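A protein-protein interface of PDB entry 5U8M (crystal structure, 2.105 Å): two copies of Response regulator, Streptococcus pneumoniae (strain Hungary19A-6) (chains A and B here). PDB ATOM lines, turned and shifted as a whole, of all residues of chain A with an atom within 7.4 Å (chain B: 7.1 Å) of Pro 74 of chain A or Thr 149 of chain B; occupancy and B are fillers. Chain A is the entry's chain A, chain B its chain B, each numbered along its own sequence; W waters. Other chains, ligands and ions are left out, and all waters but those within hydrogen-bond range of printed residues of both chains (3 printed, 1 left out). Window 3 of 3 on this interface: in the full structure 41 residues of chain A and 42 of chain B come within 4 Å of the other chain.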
ATOM      1  N   ALA A  66       0.713  31.747  19.212  1.00  0.00           N
ATOM      2  CA  ALA A  66      -0.238  31.138  18.288  1.00  0.00           C
ATOM      3  C   ALA A  66      -0.613  32.101  17.174  1.00  0.00           C
ATOM      4  O   ALA A  66      -0.737  31.698  16.013  1.00  0.00           O
ATOM      5  CB  ALA A  66      -1.492  30.698  19.044  1.00  0.00           C
ATOM      6  N   LEU A  69       2.393  32.270  14.736  1.00  0.00           N
ATOM      7  CA  LEU A  69       2.464  31.010  14.003  1.00  0.00           C
ATOM      8  C   LEU A  69       1.326  30.871  13.008  1.00  0.00           C
ATOM      9  O   LEU A  69       1.522  30.351  11.899  1.00  0.00           O
ATOM     10  CB  LEU A  69       2.446  29.840  14.977  1.00  0.00           C
ATOM     11  CG  LEU A  69       2.719  28.430  14.475  1.00  0.00           C
ATOM     12  CD1 LEU A  69       3.974  28.369  13.630  1.00  0.00           C
ATOM     13  CD2 LEU A  69       2.859  27.484  15.660  1.00  0.00           C
ATOM     14  N   SER A  70       0.125  31.302  13.388  1.00  0.00           N
ATOM     15  CA  SER A  70      -1.040  31.092  12.533  1.00  0.00           C
ATOM     16  C   SER A  70      -0.929  31.818  11.194  1.00  0.00           C
ATOM     17  O   SER A  70      -1.683  31.507  10.273  1.00  0.00           O
ATOM     18  CB  SER A  70      -2.299  31.546  13.245  1.00  0.00           C
ATOM     19  OG  SER A  70      -2.371  32.952  13.250  1.00  0.00           O
ATOM     20  N   ARG A  71      -0.024  32.786  11.065  1.00  0.00           N
ATOM     21  CA  ARG A  71       0.138  33.459   9.782  1.00  0.00           C
ATOM     22  C   ARG A  71       0.594  32.473   8.719  1.00  0.00           C
ATOM     23  O   ARG A  71       0.075  32.463   7.602  1.00  0.00           O
ATOM     24  CB  ARG A  71       1.128  34.611   9.929  1.00  0.00           C
ATOM     25  CG  ARG A  71       0.626  35.725  10.859  1.00  0.00           C
ATOM     26  CD  ARG A  71       1.770  36.598  11.367  1.00  0.00           C
ATOM     27  NE  ARG A  71       1.310  37.655  12.262  1.00  0.00           N
ATOM     28  CZ  ARG A  71       2.111  38.532  12.857  1.00  0.00           C
ATOM     29  NH1 ARG A  71       3.421  38.486  12.655  1.00  0.00           N
ATOM     30  NH2 ARG A  71       1.600  39.454  13.658  1.00  0.00           N
ATOM     31  N   THR A  72       1.516  31.604   9.071  1.00  0.00           N
ATOM     32  CA  THR A  72       2.022  30.604   8.150  1.00  0.00           C
ATOM     33  C   THR A  72       1.292  29.274   8.288  1.00  0.00           C
ATOM     34  O   THR A  72       1.066  28.587   7.293  1.00  0.00           O
ATOM     35  CB  THR A  72       3.512  30.403   8.409  1.00  0.00           C
ATOM     36  OG1 THR A  72       3.891  31.162   9.557  1.00  0.00           O
ATOM     37  CG2 THR A  72       4.285  30.887   7.263  1.00  0.00           C
ATOM     38  N   LYS A  73       0.928  28.903   9.513  1.00  0.00           N
ATOM     39  CA  LYS A  73       0.484  27.555   9.857  1.00  0.00           C
ATOM     40  C   LYS A  73      -0.781  27.645  10.714  1.00  0.00           C
ATOM     41  O   LYS A  73      -0.753  27.365  11.924  1.00  0.00           O
ATOM     42  CB  LYS A  73       1.609  26.814  10.590  1.00  0.00           C
ATOM     43  CG  LYS A  73       2.931  26.716   9.784  1.00  0.00           C
ATOM     44  CD  LYS A  73       3.973  25.817  10.459  1.00  0.00           C
ATOM     45  CE  LYS A  73       5.111  25.446   9.495  1.00  0.00           C
ATOM     46  NZ  LYS A  73       6.320  24.835  10.135  1.00  0.00           N
ATOM     47  N   PRO A  74      -1.917  28.031  10.109  1.00  0.00           N
ATOM     48  CA  PRO A  74      -3.096  28.410  10.917  1.00  0.00           C
ATOM     49  C   PRO A  74      -3.715  27.251  11.675  1.00  0.00           C
ATOM     50  O   PRO A  74      -4.386  27.477  12.695  1.00  0.00           O
ATOM     51  CB  PRO A  74      -4.078  28.978   9.875  1.00  0.00           C
ATOM     52  CG  PRO A  74      -3.632  28.371   8.560  1.00  0.00           C
ATOM     53  CD  PRO A  74      -2.137  28.234   8.668  1.00  0.00           C
ATOM     54  N   ALA A  75      -3.532  26.021  11.198  1.00  0.00           N
ATOM     55  CA  ALA A  75      -4.104  24.851  11.844  1.00  0.00           C
ATOM     56  C   ALA A  75      -3.075  24.144  12.738  1.00  0.00           C
ATOM     57  O   ALA A  75      -3.150  22.929  12.939  1.00  0.00           O
ATOM     58  CB  ALA A  75      -4.668  23.898  10.784  1.00  0.00           C
ATOM     59  N   SER A  76      -2.106  24.887  13.278  1.00  0.00           N
ATOM     60  CA  SER A  76      -1.112  24.296  14.173  1.00  0.00           C
ATOM     61  C   SER A  76      -1.794  23.666  15.389  1.00  0.00           C
ATOM     62  O   SER A  76      -2.861  24.103  15.835  1.00  0.00           O
ATOM     63  CB  SER A  76      -0.103  25.359  14.616  1.00  0.00           C
ATOM     64  OG  SER A  76       0.757  25.719  13.555  1.00  0.00           O
ATOM     65  N   VAL A  77      -1.212  22.576  15.872  1.00  0.00           N
ATOM     66  CA  VAL A  77      -1.789  21.803  16.964  1.00  0.00           C
ATOM     67  C   VAL A  77      -1.095  22.223  18.253  1.00  0.00           C
ATOM     68  O   VAL A  77       0.073  21.888  18.502  1.00  0.00           O
ATOM     69  CB  VAL A  77      -1.671  20.301  16.733  1.00  0.00           C
ATOM     70  CG1 VAL A  77      -2.293  19.591  17.895  1.00  0.00           C
ATOM     71  CG2 VAL A  77      -2.384  19.894  15.440  1.00  0.00           C
ATOM     72  N   ILE A  78      -1.805  22.979  19.073  1.00  0.00           N
ATOM     73  CA  ILE A  78      -1.228  23.574  20.267  1.00  0.00           C
ATOM     74  C   ILE A  78      -2.059  23.110  21.433  1.00  0.00           C
ATOM     75  O   ILE A  78      -3.285  23.235  21.399  1.00  0.00           O
ATOM     76  CB  ILE A  78      -1.235  25.106  20.192  1.00  0.00           C
ATOM     77  CG1 ILE A  78      -0.319  25.568  19.064  1.00  0.00           C
ATOM     78  CG2 ILE A  78      -0.846  25.681  21.497  1.00  0.00           C
ATOM     79  CD1 ILE A  78      -0.454  27.048  18.735  1.00  0.00           C
ATOM     80  N   PHE A  97      -7.496  29.242  20.470  1.00  0.00           N
ATOM     81  CA  PHE A  97      -6.295  28.852  19.731  1.00  0.00           C
ATOM     82  C   PHE A  97      -5.767  27.448  20.037  1.00  0.00           C
ATOM     83  O   PHE A  97      -4.976  26.916  19.241  1.00  0.00           O
ATOM     84  CB  PHE A  97      -5.192  29.899  19.927  1.00  0.00           C
ATOM     85  CG  PHE A  97      -4.497  29.876  21.270  1.00  0.00           C
ATOM     86  CD1 PHE A  97      -3.501  28.954  21.526  1.00  0.00           C
ATOM     87  CD2 PHE A  97      -4.777  30.830  22.229  1.00  0.00           C
ATOM     88  CE1 PHE A  97      -2.835  28.959  22.728  1.00  0.00           C
ATOM     89  CE2 PHE A  97      -4.120  30.847  23.432  1.00  0.00           C
ATOM     90  CZ  PHE A  97      -3.127  29.895  23.684  1.00  0.00           C
ATOM     91  N   ARG B 142     -11.798  27.545  -0.886  1.00  0.00           N
ATOM     92  CA  ARG B 142     -10.840  26.566  -1.375  1.00  0.00           C
ATOM     93  C   ARG B 142     -10.095  25.921  -0.213  1.00  0.00           C
ATOM     94  O   ARG B 142      -9.492  26.629   0.614  1.00  0.00           O
ATOM     95  CB  ARG B 142      -9.843  27.226  -2.329  1.00  0.00           C
ATOM     96  CG  ARG B 142     -10.400  27.438  -3.734  1.00  0.00           C
ATOM     97  CD  ARG B 142      -9.430  28.295  -4.556  1.00  0.00           C
ATOM     98  NE  ARG B 142      -9.729  28.146  -5.978  1.00  0.00           N
ATOM     99  CZ  ARG B 142      -9.105  28.811  -6.951  1.00  0.00           C
ATOM    100  NH1 ARG B 142      -9.445  28.598  -8.217  1.00  0.00           N
ATOM    101  NH2 ARG B 142      -8.132  29.663  -6.666  1.00  0.00           N
ATOM    102  N   ILE B 143     -10.096  24.584  -0.188  1.00  0.00           N
ATOM    103  CA  ILE B 143      -9.410  23.807   0.842  1.00  0.00           C
ATOM    104  C   ILE B 143      -8.084  23.294   0.292  1.00  0.00           C
ATOM    105  O   ILE B 143      -8.071  22.503  -0.658  1.00  0.00           O
ATOM    106  CB  ILE B 143     -10.258  22.622   1.323  1.00  0.00           C
ATOM    107  CG1 ILE B 143     -11.704  23.035   1.604  1.00  0.00           C
ATOM    108  CG2 ILE B 143      -9.604  21.960   2.560  1.00  0.00           C
ATOM    109  CD1 ILE B 143     -11.866  24.268   2.537  1.00  0.00           C
ATOM    110  N   ASP B 144      -6.969  23.705   0.914  1.00  0.00           N
ATOM    111  CA  ASP B 144      -5.640  23.146   0.646  1.00  0.00           C
ATOM    112  C   ASP B 144      -5.371  22.074   1.701  1.00  0.00           C
ATOM    113  O   ASP B 144      -4.953  22.358   2.835  1.00  0.00           O
ATOM    114  CB  ASP B 144      -4.573  24.242   0.626  1.00  0.00           C
ATOM    115  CG  ASP B 144      -3.145  23.703   0.334  1.00  0.00           C
ATOM    116  OD1 ASP B 144      -2.840  22.532   0.658  1.00  0.00           O
ATOM    117  OD2 ASP B 144      -2.319  24.473  -0.208  1.00  0.00           O
ATOM    118  N   VAL B 145      -5.586  20.837   1.291  1.00  0.00           N
ATOM    119  CA  VAL B 145      -5.561  19.695   2.185  1.00  0.00           C
ATOM    120  C   VAL B 145      -4.154  19.447   2.742  1.00  0.00           C
ATOM    121  O   VAL B 145      -3.993  19.149   3.931  1.00  0.00           O
ATOM    122  CB  VAL B 145      -6.124  18.496   1.414  1.00  0.00           C
ATOM    123  CG1 VAL B 145      -5.806  17.200   2.059  1.00  0.00           C
ATOM    124  CG2 VAL B 145      -7.643  18.675   1.281  1.00  0.00           C
ATOM    125  N   GLU B 146      -3.118  19.595   1.908  1.00  0.00           N
ATOM    126  CA  GLU B 146      -1.746  19.301   2.336  1.00  0.00           C
ATOM    127  C   GLU B 146      -1.247  20.292   3.374  1.00  0.00           C
ATOM    128  O   GLU B 146      -0.415  19.944   4.209  1.00  0.00           O
ATOM    129  CB  GLU B 146      -0.790  19.318   1.135  1.00  0.00           C
ATOM    130  CG  GLU B 146      -0.893  18.100   0.234  1.00  0.00           C
ATOM    131  CD  GLU B 146      -0.282  16.860   0.862  1.00  0.00           C
ATOM    132  OE1 GLU B 146       0.956  16.828   1.038  1.00  0.00           O
ATOM    133  OE2 GLU B 146      -1.041  15.924   1.188  1.00  0.00           O
ATOM    134  N   HIS B 147      -1.699  21.533   3.318  1.00  0.00           N
ATOM    135  CA  HIS B 147      -1.254  22.539   4.260  1.00  0.00           C
ATOM    136  C   HIS B 147      -2.307  22.857   5.311  1.00  0.00           C
ATOM    137  O   HIS B 147      -2.089  23.750   6.121  1.00  0.00           O
ATOM    138  CB  HIS B 147      -0.846  23.816   3.511  1.00  0.00           C
ATOM    139  CG  HIS B 147       0.178  23.577   2.446  1.00  0.00           C
ATOM    140  ND1 HIS B 147      -0.156  23.394   1.122  1.00  0.00           N
ATOM    141  CD2 HIS B 147       1.525  23.451   2.516  1.00  0.00           C
ATOM    142  CE1 HIS B 147       0.941  23.177   0.419  1.00  0.00           C
ATOM    143  NE2 HIS B 147       1.975  23.206   1.243  1.00  0.00           N
ATOM    144  N   HIS B 148      -3.441  22.160   5.315  1.00  0.00           N
ATOM    145  CA  HIS B 148      -4.491  22.418   6.296  1.00  0.00           C
ATOM    146  C   HIS B 148      -4.846  23.890   6.330  1.00  0.00           C
ATOM    147  O   HIS B 148      -4.978  24.492   7.392  1.00  0.00           O
ATOM    148  CB  HIS B 148      -4.069  21.934   7.687  1.00  0.00           C
ATOM    149  CG  HIS B 148      -3.854  20.465   7.739  1.00  0.00           C
ATOM    150  ND1 HIS B 148      -2.613  19.894   7.570  1.00  0.00           N
ATOM    151  CD2 HIS B 148      -4.732  19.441   7.861  1.00  0.00           C
ATOM    152  CE1 HIS B 148      -2.730  18.581   7.614  1.00  0.00           C
ATOM    153  NE2 HIS B 148      -4.006  18.279   7.798  1.00  0.00           N
ATOM    154  N   THR B 149      -4.962  24.484   5.151  1.00  0.00           N
ATOM    155  CA  THR B 149      -5.352  25.869   5.035  1.00  0.00           C
ATOM    156  C   THR B 149      -6.582  25.999   4.156  1.00  0.00           C
ATOM    157  O   THR B 149      -6.885  25.152   3.302  1.00  0.00           O
ATOM    158  CB  THR B 149      -4.232  26.708   4.457  1.00  0.00           C
ATOM    159  OG1 THR B 149      -3.921  26.218   3.149  1.00  0.00           O
ATOM    160  CG2 THR B 149      -3.005  26.639   5.331  1.00  0.00           C
ATOM    161  N   VAL B 150      -7.269  27.102   4.373  1.00  0.00           N
ATOM    162  CA  VAL B 150      -8.558  27.387   3.771  1.00  0.00           C
ATOM    163  C   VAL B 150      -8.480  28.805   3.240  1.00  0.00           C
ATOM    164  O   VAL B 150      -7.936  29.685   3.917  1.00  0.00           O
ATOM    165  CB  VAL B 150      -9.701  27.244   4.798  1.00  0.00           C
ATOM    166  CG1 VAL B 150     -10.979  27.782   4.247  1.00  0.00           C
ATOM    167  CG2 VAL B 150      -9.862  25.793   5.176  1.00  0.00           C
ATOM    168  N   TYR B 151      -9.002  29.018   2.027  1.00  0.00           N
ATOM    169  CA  TYR B 151      -9.063  30.336   1.413  1.00  0.00           C
ATOM    170  C   TYR B 151     -10.499  30.666   1.030  1.00  0.00           C
ATOM    171  O   TYR B 151     -11.218  29.814   0.495  1.00  0.00           O
ATOM    172  CB  TYR B 151      -8.173  30.416   0.160  1.00  0.00           C
ATOM    173  CG  TYR B 151      -6.720  30.119   0.395  1.00  0.00           C
ATOM    174  CD1 TYR B 151      -6.252  28.814   0.410  1.00  0.00           C
ATOM    175  CD2 TYR B 151      -5.810  31.141   0.584  1.00  0.00           C
ATOM    176  CE1 TYR B 151      -4.924  28.531   0.596  1.00  0.00           C
ATOM    177  CE2 TYR B 151      -4.478  30.869   0.796  1.00  0.00           C
ATOM    178  CZ  TYR B 151      -4.037  29.557   0.793  1.00  0.00           C
ATOM    179  OH  TYR B 151      -2.716  29.255   0.997  1.00  0.00           O
ATOM    180  N   MET B 156      -6.621  33.961   2.717  1.00  0.00           N
ATOM    181  CA  MET B 156      -6.469  32.848   3.660  1.00  0.00           C
ATOM    182  C   MET B 156      -7.264  33.101   4.941  1.00  0.00           C
ATOM    183  O   MET B 156      -7.064  34.114   5.615  1.00  0.00           O
ATOM    184  CB  MET B 156      -5.013  32.625   4.011  1.00  0.00           C
ATOM    185  CG  MET B 156      -4.828  31.348   4.784  1.00  0.00           C
ATOM    186  SD  MET B 156      -3.304  31.349   5.715  1.00  0.00           S
ATOM    187  CE  MET B 156      -2.155  30.621   4.565  1.00  0.00           C
ATOM    188  N   ILE B 157      -8.170  32.184   5.267  1.00  0.00           N
ATOM    189  CA  ILE B 157      -8.888  32.197   6.536  1.00  0.00           C
ATOM    190  C   ILE B 157      -8.119  31.337   7.535  1.00  0.00           C
ATOM    191  O   ILE B 157      -7.898  30.143   7.289  1.00  0.00           O
ATOM    192  CB  ILE B 157     -10.310  31.664   6.371  1.00  0.00           C
ATOM    193  CG1 ILE B 157     -10.980  32.297   5.139  1.00  0.00           C
ATOM    194  CG2 ILE B 157     -11.106  31.912   7.638  1.00  0.00           C
ATOM    195  CD1 ILE B 157     -10.992  33.821   5.167  1.00  0.00           C
ATOM    196  N   ALA B 158      -7.752  31.931   8.675  1.00  0.00           N
ATOM    197  CA  ALA B 158      -6.874  31.289   9.669  1.00  0.00           C
ATOM    198  C   ALA B 158      -7.682  30.409  10.620  1.00  0.00           C
ATOM    199  O   ALA B 158      -7.761  30.652  11.826  1.00  0.00           O
ATOM    200  CB  ALA B 158      -6.116  32.344  10.460  1.00  0.00           C
ATOM    201  N   LEU B 159      -8.263  29.356  10.062  1.00  0.00           N
ATOM    202  CA  LEU B 159      -8.929  28.363  10.891  1.00  0.00           C
ATOM    203  C   LEU B 159      -7.922  27.618  11.764  1.00  0.00           C
ATOM    204  O   LEU B 159      -6.867  27.185  11.299  1.00  0.00           O
ATOM    205  CB  LEU B 159      -9.661  27.355  10.033  1.00  0.00           C
ATOM    206  CG  LEU B 159     -10.726  27.893   9.083  1.00  0.00           C
ATOM    207  CD1 LEU B 159     -11.412  26.701   8.478  1.00  0.00           C
ATOM    208  CD2 LEU B 159     -11.747  28.774   9.817  1.00  0.00           C
ATOM    209  N   THR B 160      -8.272  27.442  13.031  1.00  0.00           N
ATOM    210  CA  THR B 160      -7.495  26.610  13.922  1.00  0.00           C
ATOM    211  C   THR B 160      -7.659  25.161  13.496  1.00  0.00           C
ATOM    212  O   THR B 160      -8.482  24.838  12.652  1.00  0.00           O
ATOM    213  CB  THR B 160      -7.978  26.770  15.350  1.00  0.00           C
ATOM    214  OG1 THR B 160      -9.304  26.237  15.423  1.00  0.00           O
ATOM    215  CG2 THR B 160      -7.983  28.237  15.744  1.00  0.00           C
ATOM    216  N   ARG B 161      -6.900  24.274  14.131  1.00  0.00           N
ATOM    217  CA  ARG B 161      -7.004  22.858  13.799  1.00  0.00           C
ATOM    218  C   ARG B 161      -8.414  22.337  14.018  1.00  0.00           C
ATOM    219  O   ARG B 161      -8.991  21.684  13.141  1.00  0.00           O
ATOM    220  CB  ARG B 161      -6.024  22.028  14.636  1.00  0.00           C
ATOM    221  CG  ARG B 161      -6.090  20.532  14.306  1.00  0.00           C
ATOM    222  CD  ARG B 161      -5.505  20.293  12.928  1.00  0.00           C
ATOM    223  NE  ARG B 161      -6.200  19.243  12.200  1.00  0.00           N
ATOM    224  CZ  ARG B 161      -5.619  18.313  11.453  1.00  0.00           C
ATOM    225  NH1 ARG B 161      -4.298  18.243  11.330  1.00  0.00           N
ATOM    226  NH2 ARG B 161      -6.379  17.423  10.848  1.00  0.00           N
ATOM    227  N   GLU B 163     -11.231  23.907  14.178  1.00  0.00           N
ATOM    228  CA  GLU B 163     -12.126  24.537  13.219  1.00  0.00           C
ATOM    229  C   GLU B 163     -11.967  23.924  11.825  1.00  0.00           C
ATOM    230  O   GLU B 163     -12.956  23.595  11.157  1.00  0.00           O
ATOM    231  CB  GLU B 163     -11.829  26.035  13.199  1.00  0.00           C
ATOM    232  CG  GLU B 163     -12.212  26.743  14.475  1.00  0.00           C
ATOM    233  CD  GLU B 163     -11.632  28.144  14.586  1.00  0.00           C
ATOM    234  OE1 GLU B 163     -10.802  28.533  13.739  1.00  0.00           O
ATOM    235  OE2 GLU B 163     -11.985  28.863  15.547  1.00  0.00           O
ATOM    236  N   TYR B 164     -10.723  23.811  11.363  1.00  0.00           N
ATOM    237  CA  TYR B 164     -10.429  23.089  10.132  1.00  0.00           C
ATOM    238  C   TYR B 164     -11.088  21.716  10.134  1.00  0.00           C
ATOM    239  O   TYR B 164     -11.778  21.343   9.173  1.00  0.00           O
ATOM    240  CB  TYR B 164      -8.910  22.958   9.939  1.00  0.00           C
ATOM    241  CG  TYR B 164      -8.569  22.286   8.643  1.00  0.00           C
ATOM    242  CD1 TYR B 164      -8.596  20.929   8.547  1.00  0.00           C
ATOM    243  CD2 TYR B 164      -8.267  23.016   7.513  1.00  0.00           C
ATOM    244  CE1 TYR B 164      -8.327  20.308   7.387  1.00  0.00           C
ATOM    245  CE2 TYR B 164      -7.962  22.396   6.337  1.00  0.00           C
ATOM    246  CZ  TYR B 164      -8.004  21.040   6.275  1.00  0.00           C
ATOM    247  OH  TYR B 164      -7.748  20.373   5.111  1.00  0.00           O
ATOM    248  N   LYS B 208     -15.186  33.066  11.537  1.00  0.00           N
ATOM    249  CA  LYS B 208     -14.022  33.196  10.667  1.00  0.00           C
ATOM    250  C   LYS B 208     -14.404  33.229   9.195  1.00  0.00           C
ATOM    251  O   LYS B 208     -13.758  33.919   8.400  1.00  0.00           O
ATOM    252  CB  LYS B 208     -13.049  32.038  10.894  1.00  0.00           C
ATOM    253  CG  LYS B 208     -12.365  32.070  12.275  1.00  0.00           C
ATOM    254  CD  LYS B 208     -10.884  32.309  12.138  1.00  0.00           C
ATOM    255  CE  LYS B 208     -10.153  32.221  13.474  1.00  0.00           C
ATOM    256  NZ  LYS B 208     -10.040  30.813  13.986  1.00  0.00           N
HETATM  257  O   HOH W   1      -2.210  25.483   9.009  1.00  0.00           O
HETATM  258  O   HOH W   2      -4.611  25.899  15.233  1.00  0.00           O
HETATM  259  O   HOH W   3      -2.102  20.275  11.668  1.00  0.00           O
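No position is printed for both chains.
Of the 10 pairs that touch across the chains among the printed residues, none has its exchanged pair printed and touching as well.
Water W2 lies within hydrogen-bond range of the backbone carbonyl oxygen of Ser 76 of chain A, the backbone carbonyl oxygen of Pro 74 of chain A and the backbone NH of Arg 161 of chain B.
Water W1 lies within hydrogen-bond range of the backbone NH of Ala 75 of chain A (2.6 Å), the backbone carbonyl oxygen of His 148 of chain B (3.4 Å) and the backbone carbonyl oxygen of His 147 of chain B (3.4 Å).
Water W3 bridges the guanidinium group (NH1) of Arg 161 of chain B (3.0 Å) and the backbone carbonyl oxygen (O) of Ala 75 of chain A (3.1 Å).
O of Lys 73 of chain A lies within hydrogen-bond range of OG of Ser 76 of chain A (2.8 Å).
The backbone NH of Asp 144 of chain B lies within hydrogen-bond range of the backbone carbonyl oxygen of Thr 149 of chain B (2.8 Å).
O of Ala 158 of chain B is in hydrogen-bond range of NZ of Lys 208 of chain B (3.1 Å).
N of Thr 160 of chain B is in hydrogen-bond range of OE1 of Glu 163 of chain B (2.8 Å).
Among the printed residues, pairs that only touch across the chains: Pro 74 of chain A with Thr 160 of chain B (3.5 Å), Ala 75 of chain A with Arg 161 of chain B (3.5 Å), Ala 75 of chain A with His 148 of chain B (3.5 Å), Ala 75 of chain A with Leu 159 of chain B (3.5 Å), Pro 74 of chain A with Ala 158 of chain B (3.6 Å), Pro 74 of chain A with Thr 149 of chain B (3.7 Å), Val 77 of chain A with Arg 161 of chain B (3.9 Å), Ala 75 of chain A with Thr 160 of chain B (3.9 Å) and Ser 76 of chain A with Arg 161 of chain B (3.97 Å).
The backbone carbonyl oxygen of Pro 74 of chain A sits close to the backbone carbonyl oxygen of Leu 159 of chain B (2.9 Å).
Hydrophobic or aromatic side chains of chain B that line the printed part of chain A: His 148 and Ala 158.
Printed residues of chain A that touch a printed residue of chain B: Pro 74, Ala 75, Ser 76 and Val 77.
Among the printed residues, no Asp or Glu carboxylate lies within 4 Å of a Lys or Arg side-chain nitrogen of the other chain.
Arg 71 of chain A touches none of the printed residues of chain B.
Pro 74 of chain A touches just these residues of chain B: Thr 149, Ala 158, Leu 159 and Thr 160.
Of the printed residues of chain B, Ser 76 of chain A touches Arg 161.
Glu 146 of chain B touches none of the printed residues of chain A.
Printed residues of chain A within 4 Å of His 148 of chain B: Ala 75 (3.5 Å).
Of chain A, only Pro 74 (3.7 Å) comes within 4 Å of Thr 149 of chain B.
The nearest residue of chain B that does not touch Pro 74 of chain A is Met 156 of chain B (4.1 Å).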
